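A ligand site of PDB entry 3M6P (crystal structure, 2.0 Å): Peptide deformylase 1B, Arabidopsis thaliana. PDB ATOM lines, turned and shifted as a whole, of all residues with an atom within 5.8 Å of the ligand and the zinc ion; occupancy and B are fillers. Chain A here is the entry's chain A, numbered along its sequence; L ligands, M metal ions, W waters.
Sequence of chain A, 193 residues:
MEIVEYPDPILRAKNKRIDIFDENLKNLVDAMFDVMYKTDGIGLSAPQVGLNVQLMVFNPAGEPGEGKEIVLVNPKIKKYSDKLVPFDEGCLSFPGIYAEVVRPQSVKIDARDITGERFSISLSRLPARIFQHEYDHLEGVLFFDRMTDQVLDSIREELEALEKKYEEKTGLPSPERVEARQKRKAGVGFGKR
A nitrogen (N1) of the ligand sits close to the backbone carbonyl oxygen of Gly 43, 3.4 Å away. O of Gly 90 lies within hydrogen-bond range of N2 of the ligand, at 3.2 Å. The backbone NH of Leu 92 sits close to an oxygen (O1) of the ligand. The backbone NH of Gly 90 lies within hydrogen-bond range of an oxygen (O4) of the ligand, 3.0 Å away. OE1 of Gln 48 lies within hydrogen-bond range of N1 of the ligand, at 3.3 Å. The side-chain carboxylate (OE2) of Glu 134 sits at hydrogen-bond distance from a nitrogen (N1) of the ligand (2.5 Å). The backbone NH (N) of Ile 42 sits at hydrogen-bond distance from an oxygen (O3) of the ligand, 2.8 Å away. The backbone carbonyl oxygen (O) of Asp 88 is in hydrogen-bond range of an oxygen (O5) of the ligand (2.6 Å).
SG of Cys 91 sits close to NE2 of Gln 48 (3.7 Å). The side-chain carboxylate (OE2) of Glu 89 lies within hydrogen-bond range of a ring nitrogen (ND1) of His 133 (2.7 Å). NE2 of Gln 48 is in hydrogen-bond range of OG of Ser 93 (3.2 Å). The backbone NH (N) of Ser 45 is in hydrogen-bond range of the side-chain carboxylate (OE1) of Glu 134 (3.2 Å). The backbone NH of Ser 45 lies within hydrogen-bond range of the side-chain amide oxygen of Gln 48 (3.0 Å). O of Phe 87 sits at hydrogen-bond distance from NH2 of Arg 129, 3.3 Å away. The backbone NH of Ser 93 lies close to the side-chain sulfur of Cys 91. The side-chain amide oxygen of Gln 48 lies close to the side-chain carboxylate of Glu 134 (3.5 Å).
Merely in contact with the ligand: Asp 40 (3.8 Å), Gly 41 (3.2 Å), Phe 87 (3.7 Å), Glu 89 (3.9 Å), Tyr 98 (3.3 Å) and Ile 130 (3.7 Å). Hydrophobic or aromatic side chains that line the ligand: Ile 42, Phe 87, Leu 92, Tyr 98, Ile 130, His 133 and His 137. Within 4 Å of the ligand: Asp 40, Gly 41, Ile 42, Gly 43, Gln 48, Phe 87, Asp 88, Glu 89, Gly 90, Cys 91, Leu 92, Tyr 98, Ile 130, His 133, Glu 134 and His 137.
NE2 of Gln 48 touches the zinc ion (3.1 Å). Of the 23 residues printed, 4 come within 4 Å of the zinc ion. The nearest printed residue that does not touch the zinc ion is Leu 92 (4.3 Å).
The zinc ion is bound by O1 of the ligand (2.1 Å), SG of Cys 91 (2.2 Å), NE2 of His 137 (2.2 Å), NE2 of His 133 (2.3 Å) and O2 of the ligand (2.4 Å). The zinc ion has five donor atoms within binding distance.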
ATOM      1  N   THR A  39      25.741  15.182  14.170  1.00  0.00           N
ATOM      2  CA  THR A  39      24.582  15.597  14.979  1.00  0.00           C
ATOM      3  C   THR A  39      24.893  15.602  16.469  1.00  0.00           C
ATOM      4  O   THR A  39      24.002  15.759  17.292  1.00  0.00           O
ATOM      5  CB  THR A  39      23.365  14.675  14.730  1.00  0.00           C
ATOM      6  OG1 THR A  39      23.741  13.305  15.046  1.00  0.00           O
ATOM      7  CG2 THR A  39      22.933  14.803  13.273  1.00  0.00           C
ATOM      8  N   ASP A  40      26.175  15.407  16.817  1.00  0.00           N
ATOM      9  CA  ASP A  40      26.607  15.240  18.218  1.00  0.00           C
ATOM     10  C   ASP A  40      25.916  14.123  19.027  1.00  0.00           C
ATOM     11  O   ASP A  40      25.673  14.273  20.245  1.00  0.00           O
ATOM     12  CB  ASP A  40      26.483  16.588  18.964  1.00  0.00           C
ATOM     13  CG  ASP A  40      27.126  17.691  18.219  1.00  0.00           C
ATOM     14  OD1 ASP A  40      28.275  17.486  17.760  1.00  0.00           O
ATOM     15  OD2 ASP A  40      26.480  18.762  18.057  1.00  0.00           O
ATOM     16  N   GLY A  41      25.701  12.970  18.385  1.00  0.00           N
ATOM     17  CA  GLY A  41      25.147  11.802  19.045  1.00  0.00           C
ATOM     18  C   GLY A  41      26.208  10.929  19.650  1.00  0.00           C
ATOM     19  O   GLY A  41      27.375  11.159  19.427  1.00  0.00           O
ATOM     20  N   ILE A  42      25.804   9.927  20.439  1.00  0.00           N
ATOM     21  CA  ILE A  42      26.727   8.980  21.005  1.00  0.00           C
ATOM     22  C   ILE A  42      26.364   7.563  20.551  1.00  0.00           C
ATOM     23  O   ILE A  42      26.967   6.613  20.964  1.00  0.00           O
ATOM     24  CB  ILE A  42      26.814   9.102  22.520  1.00  0.00           C
ATOM     25  CG1 ILE A  42      25.429   8.772  23.142  1.00  0.00           C
ATOM     26  CG2 ILE A  42      27.410  10.545  22.889  1.00  0.00           C
ATOM     27  CD1 ILE A  42      25.257   9.050  24.639  1.00  0.00           C
ATOM     28  N   GLY A  43      25.343   7.461  19.712  1.00  0.00           N
ATOM     29  CA  GLY A  43      24.984   6.251  18.999  1.00  0.00           C
ATOM     30  C   GLY A  43      23.966   6.518  17.911  1.00  0.00           C
ATOM     31  O   GLY A  43      23.415   7.641  17.810  1.00  0.00           O
ATOM     32  N   LEU A  44      23.752   5.491  17.083  1.00  0.00           N
ATOM     33  CA  LEU A  44      22.744   5.507  16.033  1.00  0.00           C
ATOM     34  C   LEU A  44      22.303   4.121  15.706  1.00  0.00           C
ATOM     35  O   LEU A  44      23.085   3.163  15.729  1.00  0.00           O
ATOM     36  CB  LEU A  44      23.247   6.223  14.719  1.00  0.00           C
ATOM     37  CG  LEU A  44      22.208   6.785  13.712  1.00  0.00           C
ATOM     38  CD1 LEU A  44      21.214   7.862  14.280  1.00  0.00           C
ATOM     39  CD2 LEU A  44      22.929   7.416  12.487  1.00  0.00           C
ATOM     40  N   SER A  45      21.028   3.986  15.330  1.00  0.00           N
ATOM     41  CA  SER A  45      20.565   2.699  14.816  1.00  0.00           C
ATOM     42  C   SER A  45      20.053   2.858  13.391  1.00  0.00           C
ATOM     43  O   SER A  45      19.560   3.930  13.010  1.00  0.00           O
ATOM     44  CB  SER A  45      19.476   2.187  15.716  1.00  0.00           C
ATOM     45  OG  SER A  45      18.328   3.008  15.567  1.00  0.00           O
ATOM     46  N   GLN A  48      16.880   4.683  12.092  1.00  0.00           N
ATOM     47  CA  GLN A  48      17.011   6.148  12.171  1.00  0.00           C
ATOM     48  C   GLN A  48      17.556   6.824  10.915  1.00  0.00           C
ATOM     49  O   GLN A  48      17.469   8.033  10.807  1.00  0.00           O
ATOM     50  CB  GLN A  48      17.836   6.555  13.365  1.00  0.00           C
ATOM     51  CG  GLN A  48      17.162   6.150  14.683  1.00  0.00           C
ATOM     52  CD  GLN A  48      17.971   6.584  15.894  1.00  0.00           C
ATOM     53  OE1 GLN A  48      18.960   5.958  16.246  1.00  0.00           O
ATOM     54  NE2 GLN A  48      17.537   7.669  16.529  1.00  0.00           N
ATOM     55  N   PHE A  87      18.719   8.109  33.968  1.00  0.00           N
ATOM     56  CA  PHE A  87      19.674   8.871  33.135  1.00  0.00           C
ATOM     57  C   PHE A  87      18.805   9.679  32.202  1.00  0.00           C
ATOM     58  O   PHE A  87      17.773   9.184  31.734  1.00  0.00           O
ATOM     59  CB  PHE A  87      20.625   7.966  32.356  1.00  0.00           C
ATOM     60  CG  PHE A  87      21.848   8.689  31.712  1.00  0.00           C
ATOM     61  CD1 PHE A  87      22.871   9.222  32.500  1.00  0.00           C
ATOM     62  CD2 PHE A  87      21.963   8.802  30.325  1.00  0.00           C
ATOM     63  CE1 PHE A  87      23.987   9.848  31.922  1.00  0.00           C
ATOM     64  CE2 PHE A  87      23.078   9.443  29.730  1.00  0.00           C
ATOM     65  CZ  PHE A  87      24.077   9.956  30.513  1.00  0.00           C
ATOM     66  N   ASP A  88      19.177  10.934  31.983  1.00  0.00           N
ATOM     67  CA  ASP A  88      18.479  11.801  31.041  1.00  0.00           C
ATOM     68  C   ASP A  88      18.902  11.483  29.620  1.00  0.00           C
ATOM     69  O   ASP A  88      20.050  11.693  29.244  1.00  0.00           O
ATOM     70  CB  ASP A  88      18.736  13.262  31.358  1.00  0.00           C
ATOM     71  CG  ASP A  88      18.102  13.664  32.635  1.00  0.00           C
ATOM     72  OD1 ASP A  88      17.979  14.881  32.893  1.00  0.00           O
ATOM     73  OD2 ASP A  88      17.701  12.756  33.403  1.00  0.00           O
ATOM     74  N   GLU A  89      17.941  10.976  28.853  1.00  0.00           N
ATOM     75  CA  GLU A  89      18.156  10.628  27.448  1.00  0.00           C
ATOM     76  C   GLU A  89      17.508  11.635  26.561  1.00  0.00           C
ATOM     77  O   GLU A  89      16.456  12.178  26.897  1.00  0.00           O
ATOM     78  CB  GLU A  89      17.502   9.286  27.131  1.00  0.00           C
ATOM     79  CG  GLU A  89      17.686   8.250  28.191  1.00  0.00           C
ATOM     80  CD  GLU A  89      17.653   6.832  27.663  1.00  0.00           C
ATOM     81  OE1 GLU A  89      18.034   5.934  28.441  1.00  0.00           O
ATOM     82  OE2 GLU A  89      17.232   6.612  26.490  1.00  0.00           O
ATOM     83  N   GLY A  90      18.145  11.851  25.411  1.00  0.00           N
ATOM     84  CA  GLY A  90      17.543  12.483  24.262  1.00  0.00           C
ATOM     85  C   GLY A  90      17.623  11.491  23.120  1.00  0.00           C
ATOM     86  O   GLY A  90      18.355  10.498  23.167  1.00  0.00           O
ATOM     87  N   CYS A  91      17.026  11.826  22.011  1.00  0.00           N
ATOM     88  CA  CYS A  91      17.087  10.912  20.901  1.00  0.00           C
ATOM     89  C   CYS A  91      17.102  11.741  19.662  1.00  0.00           C
ATOM     90  O   CYS A  91      16.357  12.710  19.548  1.00  0.00           O
ATOM     91  CB  CYS A  91      15.850   9.966  20.943  1.00  0.00           C
ATOM     92  SG  CYS A  91      15.734   8.693  19.645  1.00  0.00           S
ATOM     93  N   LEU A  92      17.964  11.361  18.720  1.00  0.00           N
ATOM     94  CA  LEU A  92      18.078  12.056  17.413  1.00  0.00           C
ATOM     95  C   LEU A  92      16.776  12.038  16.608  1.00  0.00           C
ATOM     96  O   LEU A  92      16.549  12.897  15.720  1.00  0.00           O
ATOM     97  CB  LEU A  92      19.217  11.449  16.593  1.00  0.00           C
ATOM     98  CG  LEU A  92      20.607  11.958  17.053  1.00  0.00           C
ATOM     99  CD1 LEU A  92      21.648  11.351  16.186  1.00  0.00           C
ATOM    100  CD2 LEU A  92      20.726  13.453  17.034  1.00  0.00           C
ATOM    101  N   SER A  93      15.912  11.076  16.904  1.00  0.00           N
ATOM    102  CA  SER A  93      14.614  11.020  16.231  1.00  0.00           C
ATOM    103  C   SER A  93      13.577  11.886  16.877  1.00  0.00           C
ATOM    104  O   SER A  93      12.430  11.880  16.469  1.00  0.00           O
ATOM    105  CB  SER A  93      14.072   9.612  16.167  1.00  0.00           C
ATOM    106  OG  SER A  93      14.838   8.856  15.222  1.00  0.00           O
ATOM    107  N   ILE A  97      14.170  16.960  22.510  1.00  0.00           N
ATOM    108  CA  ILE A  97      13.390  16.374  23.621  1.00  0.00           C
ATOM    109  C   ILE A  97      14.295  15.566  24.512  1.00  0.00           C
ATOM    110  O   ILE A  97      14.959  14.675  23.999  1.00  0.00           O
ATOM    111  CB  ILE A  97      12.180  15.518  23.105  1.00  0.00           C
ATOM    112  CG1 ILE A  97      11.239  16.379  22.224  1.00  0.00           C
ATOM    113  CG2 ILE A  97      11.422  14.810  24.329  1.00  0.00           C
ATOM    114  CD1 ILE A  97      10.100  15.591  21.648  1.00  0.00           C
ATOM    115  N   TYR A  98      14.365  15.885  25.808  1.00  0.00           N
ATOM    116  CA  TYR A  98      15.229  15.214  26.793  1.00  0.00           C
ATOM    117  C   TYR A  98      14.396  14.838  28.012  1.00  0.00           C
ATOM    118  O   TYR A  98      13.587  15.632  28.467  1.00  0.00           O
ATOM    119  CB  TYR A  98      16.404  16.124  27.249  1.00  0.00           C
ATOM    120  CG  TYR A  98      17.316  16.546  26.110  1.00  0.00           C
ATOM    121  CD1 TYR A  98      17.035  17.672  25.332  1.00  0.00           C
ATOM    122  CD2 TYR A  98      18.446  15.793  25.793  1.00  0.00           C
ATOM    123  CE1 TYR A  98      17.835  18.030  24.232  1.00  0.00           C
ATOM    124  CE2 TYR A  98      19.273  16.147  24.720  1.00  0.00           C
ATOM    125  CZ  TYR A  98      18.956  17.258  23.930  1.00  0.00           C
ATOM    126  OH  TYR A  98      19.791  17.592  22.856  1.00  0.00           O
ATOM    127  N   LEU A 126      27.849   3.914  30.621  1.00  0.00           N
ATOM    128  CA  LEU A 126      27.286   4.563  29.438  1.00  0.00           C
ATOM    129  C   LEU A 126      27.146   3.539  28.318  1.00  0.00           C
ATOM    130  O   LEU A 126      26.112   3.455  27.665  1.00  0.00           O
ATOM    131  CB  LEU A 126      28.116   5.791  29.028  1.00  0.00           C
ATOM    132  CG  LEU A 126      27.479   6.871  28.120  1.00  0.00           C
ATOM    133  CD1 LEU A 126      26.178   7.424  28.648  1.00  0.00           C
ATOM    134  CD2 LEU A 126      28.434   8.004  27.922  1.00  0.00           C
ATOM    135  N   ARG A 129      23.898   1.853  28.748  1.00  0.00           N
ATOM    136  CA  ARG A 129      22.807   2.818  28.562  1.00  0.00           C
ATOM    137  C   ARG A 129      22.544   3.121  27.030  1.00  0.00           C
ATOM    138  O   ARG A 129      21.415   3.099  26.554  1.00  0.00           O
ATOM    139  CB  ARG A 129      23.172   4.083  29.293  1.00  0.00           C
ATOM    140  CG  ARG A 129      22.036   5.048  29.343  1.00  0.00           C
ATOM    141  CD  ARG A 129      20.877   4.235  29.933  1.00  0.00           C
ATOM    142  NE  ARG A 129      19.778   5.049  30.289  1.00  0.00           N
ATOM    143  CZ  ARG A 129      19.161   5.073  31.431  1.00  0.00           C
ATOM    144  NH1 ARG A 129      19.483   4.271  32.437  1.00  0.00           N
ATOM    145  NH2 ARG A 129      18.170   5.946  31.525  1.00  0.00           N
ATOM    146  N   ILE A 130      23.602   3.383  26.287  1.00  0.00           N
ATOM    147  CA  ILE A 130      23.490   3.665  24.870  1.00  0.00           C
ATOM    148  C   ILE A 130      22.964   2.416  24.160  1.00  0.00           C
ATOM    149  O   ILE A 130      22.042   2.494  23.316  1.00  0.00           O
ATOM    150  CB  ILE A 130      24.867   4.025  24.268  1.00  0.00           C
ATOM    151  CG1 ILE A 130      25.441   5.304  24.897  1.00  0.00           C
ATOM    152  CG2 ILE A 130      24.763   4.157  22.770  1.00  0.00           C
ATOM    153  CD1 ILE A 130      26.911   5.570  24.502  1.00  0.00           C
ATOM    154  N   HIS A 133      19.180   1.843  24.792  1.00  0.00           N
ATOM    155  CA  HIS A 133      18.558   2.842  23.874  1.00  0.00           C
ATOM    156  C   HIS A 133      18.474   2.413  22.379  1.00  0.00           C
ATOM    157  O   HIS A 133      17.393   2.439  21.768  1.00  0.00           O
ATOM    158  CB  HIS A 133      19.260   4.180  23.947  1.00  0.00           C
ATOM    159  CG  HIS A 133      18.539   5.268  23.217  1.00  0.00           C
ATOM    160  ND1 HIS A 133      17.787   6.230  23.872  1.00  0.00           N
ATOM    161  CD2 HIS A 133      18.459   5.558  21.894  1.00  0.00           C
ATOM    162  CE1 HIS A 133      17.291   7.072  22.966  1.00  0.00           C
ATOM    163  NE2 HIS A 133      17.658   6.653  21.765  1.00  0.00           N
ATOM    164  N   GLU A 134      19.609   1.995  21.814  1.00  0.00           N
ATOM    165  CA  GLU A 134      19.712   1.641  20.382  1.00  0.00           C
ATOM    166  C   GLU A 134      19.095   0.242  20.091  1.00  0.00           C
ATOM    167  O   GLU A 134      18.531  -0.003  19.034  1.00  0.00           O
ATOM    168  CB  GLU A 134      21.157   1.599  19.924  1.00  0.00           C
ATOM    169  CG  GLU A 134      22.038   2.772  20.131  1.00  0.00           C
ATOM    170  CD  GLU A 134      21.502   4.045  19.505  1.00  0.00           C
ATOM    171  OE1 GLU A 134      20.765   3.986  18.472  1.00  0.00           O
ATOM    172  OE2 GLU A 134      21.867   5.119  20.025  1.00  0.00           O
ATOM    173  N   HIS A 137      15.617   0.565  19.646  1.00  0.00           N
ATOM    174  CA  HIS A 137      15.319   0.979  18.290  1.00  0.00           C
ATOM    175  C   HIS A 137      15.240  -0.223  17.335  1.00  0.00           C
ATOM    176  O   HIS A 137      14.413  -0.261  16.414  1.00  0.00           O
ATOM    177  CB  HIS A 137      16.378   1.953  17.803  1.00  0.00           C
ATOM    178  CG  HIS A 137      16.104   3.398  18.139  1.00  0.00           C
ATOM    179  ND1 HIS A 137      15.043   4.093  17.610  1.00  0.00           N
ATOM    180  CD2 HIS A 137      16.860   4.306  18.803  1.00  0.00           C
ATOM    181  CE1 HIS A 137      15.076   5.347  18.034  1.00  0.00           C
ATOM    182  NE2 HIS A 137      16.199   5.530  18.706  1.00  0.00           N
HETATM  183  C1  LIG L   1      21.218   9.055  19.545  1.00  0.00           C
HETATM  184  C2  LIG L   1      20.081   8.127  19.266  1.00  0.00           C
HETATM  185  O1  LIG L   1      18.963   8.583  19.263  1.00  0.00           O
HETATM  186  N1  LIG L   1      20.368   6.836  19.079  1.00  0.00           N
HETATM  187  O2  LIG L   1      19.296   6.015  18.850  1.00  0.00           O
HETATM  188  C3  LIG L   1      21.043   9.303  21.051  1.00  0.00           C
HETATM  189  C4  LIG L   1      21.938  10.413  21.498  1.00  0.00           C
HETATM  190  O3  LIG L   1      23.104  10.480  21.101  1.00  0.00           O
HETATM  191  C5  LIG L   1      21.536   8.017  21.860  1.00  0.00           C
HETATM  192  C6  LIG L   1      21.525   8.244  23.407  1.00  0.00           C
HETATM  193  C7  LIG L   1      22.010   7.017  24.132  1.00  0.00           C
HETATM  194  C8  LIG L   1      21.502   7.083  25.639  1.00  0.00           C
HETATM  195  C9  LIG L   1      21.831   8.431  26.346  1.00  0.00           C
HETATM  196  N2  LIG L   1      21.373  11.241  22.327  1.00  0.00           N
HETATM  197  C10 LIG L   1      22.144  12.319  22.913  1.00  0.00           C
HETATM  198  C11 LIG L   1      21.663  13.700  22.461  1.00  0.00           C
HETATM  199  C12 LIG L   1      21.955  13.856  20.933  1.00  0.00           C
HETATM  200  C13 LIG L   1      20.194  13.802  22.652  1.00  0.00           C
HETATM  201  C14 LIG L   1      22.101  12.119  24.459  1.00  0.00           C
HETATM  202  O4  LIG L   1      21.099  11.630  25.008  1.00  0.00           O
HETATM  203  N3  LIG L   1      23.192  12.457  25.211  1.00  0.00           N
HETATM  204  C15 LIG L   1      23.262  12.308  26.664  1.00  0.00           C
HETATM  205  C16 LIG L   1      24.454  13.017  24.680  1.00  0.00           C
HETATM  206  C17 LIG L   1      25.493  12.638  25.737  1.00  0.00           C
HETATM  207  C18 LIG L   1      24.716  12.587  27.040  1.00  0.00           C
HETATM  208  C19 LIG L   1      22.374  13.358  27.385  1.00  0.00           C
HETATM  209  O5  LIG L   1      22.283  12.923  28.749  1.00  0.00           O
HETATM  210 ZN    ZN M   1      17.389   7.209  19.578  1.00  0.00          ZN
HETATM  211  O   HOH W   1      27.395  15.423  25.149  1.00  0.00           O
HETATM  212  O   HOH W   2      24.160  13.540  30.897  1.00  0.00           O
